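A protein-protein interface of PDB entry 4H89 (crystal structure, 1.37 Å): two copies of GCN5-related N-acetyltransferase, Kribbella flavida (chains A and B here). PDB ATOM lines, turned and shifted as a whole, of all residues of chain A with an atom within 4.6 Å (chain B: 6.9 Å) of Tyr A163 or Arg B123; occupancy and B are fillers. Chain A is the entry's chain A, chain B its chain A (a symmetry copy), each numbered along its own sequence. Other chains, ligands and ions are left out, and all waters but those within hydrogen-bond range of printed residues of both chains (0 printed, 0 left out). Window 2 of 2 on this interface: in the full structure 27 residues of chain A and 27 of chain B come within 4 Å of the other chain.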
ATOM      1  N   GLU A 154      21.706   9.634 -11.018  1.00  0.00           N
ATOM      2  CA  GLU A 154      22.608   8.530 -10.695  1.00  0.00           C
ATOM      3  C   GLU A 154      22.110   7.181 -11.209  1.00  0.00           C
ATOM      4  O   GLU A 154      22.396   6.144 -10.630  1.00  0.00           O
ATOM      5  CB  GLU A 154      22.881   8.509  -9.178  1.00  0.00           C
ATOM      6  CG  GLU A 154      23.709   9.686  -8.700  1.00  0.00           C
ATOM      7  CD  GLU A 154      24.223   9.528  -7.301  1.00  0.00           C
ATOM      8  OE1 GLU A 154      25.287  10.082  -7.028  1.00  0.00           O
ATOM      9  OE2 GLU A 154      23.551   8.984  -6.463  1.00  0.00           O
ATOM     10  N   PHE A 156      22.983   5.693 -14.114  1.00  0.00           N
ATOM     11  CA  PHE A 156      23.868   5.046 -15.085  1.00  0.00           C
ATOM     12  C   PHE A 156      25.286   5.177 -14.578  1.00  0.00           C
ATOM     13  O   PHE A 156      25.715   6.276 -14.251  1.00  0.00           O
ATOM     14  CB  PHE A 156      23.736   5.767 -16.450  1.00  0.00           C
ATOM     15  CG  PHE A 156      24.523   5.134 -17.581  1.00  0.00           C
ATOM     16  CD1 PHE A 156      25.847   5.490 -17.804  1.00  0.00           C
ATOM     17  CD2 PHE A 156      23.950   4.210 -18.427  1.00  0.00           C
ATOM     18  CE1 PHE A 156      26.533   4.922 -18.856  1.00  0.00           C
ATOM     19  CE2 PHE A 156      24.629   3.661 -19.481  1.00  0.00           C
ATOM     20  CZ  PHE A 156      25.922   4.013 -19.696  1.00  0.00           C
ATOM     21  N   HIS A 157      26.026   4.068 -14.471  1.00  0.00           N
ATOM     22  CA  HIS A 157      27.449   4.116 -14.051  1.00  0.00           C
ATOM     23  C   HIS A 157      28.347   4.324 -15.267  1.00  0.00           C
ATOM     24  O   HIS A 157      28.460   3.475 -16.133  1.00  0.00           O
ATOM     25  CB  HIS A 157      27.862   2.854 -13.302  1.00  0.00           C
ATOM     26  CG  HIS A 157      29.222   3.012 -12.708  1.00  0.00           C
ATOM     27  ND1 HIS A 157      30.367   2.597 -13.331  1.00  0.00           N
ATOM     28  CD2 HIS A 157      29.613   3.659 -11.596  1.00  0.00           C
ATOM     29  CE1 HIS A 157      31.419   2.992 -12.633  1.00  0.00           C
ATOM     30  NE2 HIS A 157      30.990   3.618 -11.556  1.00  0.00           N
ATOM     31  N   HIS A 161      32.863   9.191 -15.295  1.00  0.00           N
ATOM     32  CA  HIS A 161      32.144  10.245 -14.554  1.00  0.00           C
ATOM     33  C   HIS A 161      31.348   9.718 -13.388  1.00  0.00           C
ATOM     34  O   HIS A 161      30.689  10.497 -12.688  1.00  0.00           O
ATOM     35  CB  HIS A 161      31.237  11.044 -15.497  1.00  0.00           C
ATOM     36  CG  HIS A 161      31.982  11.629 -16.634  1.00  0.00           C
ATOM     37  ND1 HIS A 161      33.170  12.318 -16.465  1.00  0.00           N
ATOM     38  CD2 HIS A 161      31.751  11.588 -17.958  1.00  0.00           C
ATOM     39  CE1 HIS A 161      33.622  12.675 -17.645  1.00  0.00           C
ATOM     40  NE2 HIS A 161      32.771  12.264 -18.565  1.00  0.00           N
ATOM     41  N   GLY A 162      31.381   8.398 -13.181  1.00  0.00           N
ATOM     42  CA  GLY A 162      30.698   7.781 -12.065  1.00  0.00           C
ATOM     43  C   GLY A 162      29.200   7.667 -12.321  1.00  0.00           C
ATOM     44  O   GLY A 162      28.754   7.586 -13.482  1.00  0.00           O
ATOM     45  N   TYR A 163      28.439   7.648 -11.248  1.00  0.00           N
ATOM     46  CA  TYR A 163      26.990   7.553 -11.394  1.00  0.00           C
ATOM     47  C   TYR A 163      26.434   8.891 -11.886  1.00  0.00           C
ATOM     48  O   TYR A 163      26.647   9.919 -11.253  1.00  0.00           O
ATOM     49  CB  TYR A 163      26.287   7.145 -10.105  1.00  0.00           C
ATOM     50  CG  TYR A 163      26.615   5.742  -9.650  1.00  0.00           C
ATOM     51  CD1 TYR A 163      26.037   4.636 -10.260  1.00  0.00           C
ATOM     52  CD2 TYR A 163      27.522   5.503  -8.628  1.00  0.00           C
ATOM     53  CE1 TYR A 163      26.335   3.351  -9.845  1.00  0.00           C
ATOM     54  CE2 TYR A 163      27.816   4.220  -8.210  1.00  0.00           C
ATOM     55  CZ  TYR A 163      27.242   3.154  -8.807  1.00  0.00           C
ATOM     56  OH  TYR A 163      27.518   1.867  -8.442  1.00  0.00           O
ATOM     57  N   VAL A 164      25.789   8.866 -13.038  1.00  0.00           N
ATOM     58  CA  VAL A 164      25.241  10.044 -13.707  1.00  0.00           C
ATOM     59  C   VAL A 164      23.771   9.806 -14.080  1.00  0.00           C
ATOM     60  O   VAL A 164      23.228   8.682 -14.029  1.00  0.00           O
ATOM     61  CB  VAL A 164      26.068  10.426 -14.954  1.00  0.00           C
ATOM     62  CG1 VAL A 164      27.506  10.693 -14.550  1.00  0.00           C
ATOM     63  CG2 VAL A 164      26.001   9.383 -16.049  1.00  0.00           C
ATOM     64  N   PRO B  85      25.314  -1.224 -16.990  1.00  0.00           N
ATOM     65  CA  PRO B  85      25.603  -0.045 -16.189  1.00  0.00           C
ATOM     66  C   PRO B  85      24.383   0.665 -15.637  1.00  0.00           C
ATOM     67  O   PRO B  85      24.533   1.640 -14.927  1.00  0.00           O
ATOM     68  CB  PRO B  85      26.376   0.845 -17.162  1.00  0.00           C
ATOM     69  CG  PRO B  85      25.835   0.482 -18.498  1.00  0.00           C
ATOM     70  CD  PRO B  85      25.596  -0.998 -18.408  1.00  0.00           C
ATOM     71  N   ALA B  87      22.041  -1.410 -13.918  1.00  0.00           N
ATOM     72  CA  ALA B  87      21.438  -2.466 -13.154  1.00  0.00           C
ATOM     73  C   ALA B  87      21.312  -2.180 -11.635  1.00  0.00           C
ATOM     74  O   ALA B  87      20.737  -2.962 -10.891  1.00  0.00           O
ATOM     75  CB  ALA B  87      22.166  -3.751 -13.385  1.00  0.00           C
ATOM     76  N   HIS B  88      21.928  -1.092 -11.168  1.00  0.00           N
ATOM     77  CA  HIS B  88      21.834  -0.697  -9.782  1.00  0.00           C
ATOM     78  C   HIS B  88      20.524   0.023  -9.429  1.00  0.00           C
ATOM     79  O   HIS B  88      20.291   0.344  -8.267  1.00  0.00           O
ATOM     80  CB  HIS B  88      23.022   0.212  -9.414  1.00  0.00           C
ATOM     81  CG  HIS B  88      23.102   1.423 -10.252  1.00  0.00           C
ATOM     82  ND1 HIS B  88      23.522   1.383 -11.561  1.00  0.00           N
ATOM     83  CD2 HIS B  88      22.710   2.686 -10.006  1.00  0.00           C
ATOM     84  CE1 HIS B  88      23.425   2.589 -12.084  1.00  0.00           C
ATOM     85  NE2 HIS B  88      22.931   3.398 -11.150  1.00  0.00           N
ATOM     86  N   VAL B  89      19.679   0.222 -10.445  1.00  0.00           N
ATOM     87  CA  VAL B  89      18.365   0.784 -10.230  1.00  0.00           C
ATOM     88  C   VAL B  89      17.353  -0.360 -10.446  1.00  0.00           C
ATOM     89  O   VAL B  89      17.336  -0.955 -11.520  1.00  0.00           O
ATOM     90  CB  VAL B  89      18.069   1.928 -11.209  1.00  0.00           C
ATOM     91  CG1 VAL B  89      16.699   2.516 -10.941  1.00  0.00           C
ATOM     92  CG2 VAL B  89      19.118   3.019 -11.131  1.00  0.00           C
ATOM     93  N   ALA B  90      16.545  -0.646  -9.428  1.00  0.00           N
ATOM     94  CA  ALA B  90      15.501  -1.660  -9.531  1.00  0.00           C
ATOM     95  C   ALA B  90      14.239  -1.042 -10.098  1.00  0.00           C
ATOM     96  O   ALA B  90      14.069   0.166 -10.123  1.00  0.00           O
ATOM     97  CB  ALA B  90      15.194  -2.162  -8.122  1.00  0.00           C
ATOM     98  N   ALA B 117      14.773  -4.672  -2.291  1.00  0.00           N
ATOM     99  CA  ALA B 117      15.734  -3.951  -3.130  1.00  0.00           C
ATOM    100  C   ALA B 117      16.868  -3.465  -2.265  1.00  0.00           C
ATOM    101  O   ALA B 117      18.030  -3.436  -2.697  1.00  0.00           O
ATOM    102  CB  ALA B 117      15.042  -2.801  -3.846  1.00  0.00           C
ATOM    103  N   GLY B 121      20.962  -4.725  -2.423  1.00  0.00           N
ATOM    104  CA  GLY B 121      22.039  -3.833  -2.773  1.00  0.00           C
ATOM    105  C   GLY B 121      21.772  -2.793  -3.833  1.00  0.00           C
ATOM    106  O   GLY B 121      22.664  -2.034  -4.200  1.00  0.00           O
ATOM    107  N   PHE B 122      20.520  -2.667  -4.271  1.00  0.00           N
ATOM    108  CA  PHE B 122      20.208  -1.649  -5.257  1.00  0.00           C
ATOM    109  C   PHE B 122      20.406  -0.274  -4.621  1.00  0.00           C
ATOM    110  O   PHE B 122      20.283  -0.090  -3.404  1.00  0.00           O
ATOM    111  CB  PHE B 122      18.763  -1.822  -5.754  1.00  0.00           C
ATOM    112  CG  PHE B 122      18.533  -3.030  -6.651  1.00  0.00           C
ATOM    113  CD1 PHE B 122      18.771  -2.970  -7.994  1.00  0.00           C
ATOM    114  CD2 PHE B 122      18.119  -4.214  -6.106  1.00  0.00           C
ATOM    115  CE1 PHE B 122      18.499  -4.041  -8.836  1.00  0.00           C
ATOM    116  CE2 PHE B 122      17.804  -5.296  -6.930  1.00  0.00           C
ATOM    117  CZ  PHE B 122      18.030  -5.229  -8.295  1.00  0.00           C
ATOM    118  N   ARG B 123      20.632   0.711  -5.482  1.00  0.00           N
ATOM    119  CA  ARG B 123      20.828   2.109  -5.075  1.00  0.00           C
ATOM    120  C   ARG B 123      19.570   2.980  -5.212  1.00  0.00           C
ATOM    121  O   ARG B 123      19.502   4.051  -4.632  1.00  0.00           O
ATOM    122  CB  ARG B 123      21.933   2.748  -5.879  1.00  0.00           C
ATOM    123  CG  ARG B 123      23.285   2.258  -5.473  1.00  0.00           C
ATOM    124  CD  ARG B 123      24.387   2.729  -6.399  1.00  0.00           C
ATOM    125  NE  ARG B 123      25.700   2.764  -5.757  1.00  0.00           N
ATOM    126  CZ  ARG B 123      26.454   1.697  -5.524  1.00  0.00           C
ATOM    127  NH1 ARG B 123      27.636   1.916  -5.044  1.00  0.00           N
ATOM    128  NH2 ARG B 123      26.060   0.411  -5.764  1.00  0.00           N
ATOM    129  N   ALA B 124      18.567   2.506  -5.950  1.00  0.00           N
ATOM    130  CA  ALA B 124      17.350   3.257  -6.206  1.00  0.00           C
ATOM    131  C   ALA B 124      16.335   2.326  -6.838  1.00  0.00           C
ATOM    132  O   ALA B 124      16.655   1.219  -7.214  1.00  0.00           O
ATOM    133  CB  ALA B 124      17.643   4.435  -7.115  1.00  0.00           C
ATOM    134  N   ILE B 125      15.123   2.851  -6.918  1.00  0.00           N
ATOM    135  CA  ILE B 125      14.007   2.202  -7.598  1.00  0.00           C
ATOM    136  C   ILE B 125      13.359   3.218  -8.537  1.00  0.00           C
ATOM    137  O   ILE B 125      13.174   4.370  -8.186  1.00  0.00           O
ATOM    138  CB  ILE B 125      12.925   1.721  -6.621  1.00  0.00           C
ATOM    139  CG1 ILE B 125      13.517   0.878  -5.503  1.00  0.00           C
ATOM    140  CG2 ILE B 125      11.859   0.899  -7.335  1.00  0.00           C
ATOM    141  CD1 ILE B 125      12.609   0.663  -4.299  1.00  0.00           C
ATOM    142  N   HIS B 170      10.614   7.828  -8.943  1.00  0.00           N
ATOM    143  CA  HIS B 170      11.912   7.384  -8.455  1.00  0.00           C
ATOM    144  C   HIS B 170      11.998   7.513  -6.958  1.00  0.00           C
ATOM    145  O   HIS B 170      11.414   8.415  -6.357  1.00  0.00           O
ATOM    146  CB  HIS B 170      12.972   8.256  -9.101  1.00  0.00           C
ATOM    147  CG  HIS B 170      14.370   8.031  -8.605  1.00  0.00           C
ATOM    148  ND1 HIS B 170      14.903   8.783  -7.591  1.00  0.00           N
ATOM    149  CD2 HIS B 170      15.350   7.166  -8.988  1.00  0.00           C
ATOM    150  CE1 HIS B 170      16.145   8.412  -7.377  1.00  0.00           C
ATOM    151  NE2 HIS B 170      16.444   7.455  -8.227  1.00  0.00           N
ATOM    152  N   ARG B 171      12.737   6.594  -6.340  1.00  0.00           N
ATOM    153  CA  ARG B 171      13.009   6.605  -4.890  1.00  0.00           C
ATOM    154  C   ARG B 171      14.473   6.198  -4.724  1.00  0.00           C
ATOM    155  O   ARG B 171      14.858   5.164  -5.272  1.00  0.00           O
ATOM    156  CB  ARG B 171      12.127   5.527  -4.238  1.00  0.00           C
ATOM    157  CG  ARG B 171      12.137   5.515  -2.734  1.00  0.00           C
ATOM    158  CD  ARG B 171      11.456   4.271  -2.232  1.00  0.00           C
ATOM    159  NE  ARG B 171      11.051   4.354  -0.836  1.00  0.00           N
ATOM    160  CZ  ARG B 171      11.869   4.246   0.192  1.00  0.00           C
ATOM    161  NH1 ARG B 171      13.185   4.145   0.039  1.00  0.00           N
ATOM    162  NH2 ARG B 171      11.358   4.245   1.390  1.00  0.00           N
ATOM    163  N   PRO B 172      15.303   6.972  -3.966  1.00  0.00           N
ATOM    164  CA  PRO B 172      16.609   6.468  -3.588  1.00  0.00           C
ATOM    165  C   PRO B 172      16.510   5.377  -2.532  1.00  0.00           C
ATOM    166  O   PRO B 172      15.522   5.307  -1.802  1.00  0.00           O
ATOM    167  CB  PRO B 172      17.329   7.697  -3.017  1.00  0.00           C
ATOM    168  CG  PRO B 172      16.213   8.487  -2.414  1.00  0.00           C
ATOM    169  CD  PRO B 172      15.038   8.294  -3.374  1.00  0.00           C
ATOM    170  N   LEU B 173      17.527   4.522  -2.461  1.00  0.00           N
ATOM    171  CA  LEU B 173      17.689   3.539  -1.407  1.00  0.00           C
ATOM    172  C   LEU B 173      19.007   3.796  -0.691  1.00  0.00           C
ATOM    173  O   LEU B 173      19.215   3.284   0.402  1.00  0.00           O
ATOM    174  CB  LEU B 173      17.718   2.134  -1.986  1.00  0.00           C
ATOM    175  CG  LEU B 173      16.430   1.645  -2.608  1.00  0.00           C
ATOM    176  CD1 LEU B 173      16.719   0.370  -3.380  1.00  0.00           C
ATOM    177  CD2 LEU B 173      15.342   1.426  -1.566  1.00  0.00           C
ATOM    178  OXT LEU B 173      19.879   4.482  -1.226  1.00  0.00           O
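Among the printed residues, pairs that only touch across the chains: Phe A156 with Pro B85 (3.5 Å), Phe A156 with His B88 (3.7 Å), His A157 with His B88 (3.8 Å) and Tyr A163 with His B88 (3.5 Å).
The backbone carbonyl oxygen of Phe A156 lies within hydrogen-bond range of the backbone NH of Val A164, at 2.9 Å. The backbone carbonyl oxygen (O) of His B88 is in hydrogen-bond range of the backbone NH (N) of Arg B123, 2.8 Å away. The backbone carbonyl oxygen (O) of Arg B123 is in hydrogen-bond range of the backbone NH (N) of Leu B173, at 3.0 Å.
A ring nitrogen (NE2) of His B88 sits at hydrogen-bond distance from the backbone carbonyl oxygen (O) of Glu A154, at 2.8 Å. The backbone carbonyl oxygen (O) of Pro B85 lies within hydrogen-bond range of the backbone NH (N) of His A157 (2.9 Å). The side-chain hydroxyl (OH) of Tyr A163 lies close to the guanidinium group (NE) of Arg B123 (3.4 Å).
No position is printed for both chains.
Of the 15 printed residues of chain B, 3 touch a printed residue of chain A. Hydrophobic or aromatic side chains of chain B that line the printed part of chain A: Pro B85 and His B88. Of the 7 printed residues of chain A, 4 touch a printed residue of chain B. Printed residues of chain A that touch a printed residue of chain B: Glu A154, Phe A156, His A157 and Tyr A163. Hydrophobic or aromatic side chains of chain A that line the printed part of chain B: Phe A156, His A157 and Tyr A163. Among the printed residues, no Asp or Glu carboxylate lies within 4 Å of a Lys or Arg side-chain nitrogen of the other chain.
Of the printed residues of chain B, Tyr A163 touches His B88 (3.5 Å) and Arg B123 (3.1 Å). Of the printed residues of chain A, Pro B85 touches Phe A156 (3.5 Å) and His A157 (2.9 Å). Printed residues of chain B within 4 Å of His A157: Pro B85 (2.9 Å) and His B88 (3.8 Å). Of the printed residues of chain B, Phe A156 touches Pro B85 and His B88. Printed residues of chain A within 4 Å of His B88: Glu A154 (2.8 Å), Phe A156 (3.7 Å), His A157 (3.8 Å) and Tyr A163 (3.5 Å). Arg B171 touches none of the printed residues of chain A. Ala B90 touches none of the printed residues of chain A. The nearest residue of chain B that does not touch Tyr A163 is Pro B85 (5.7 Å).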
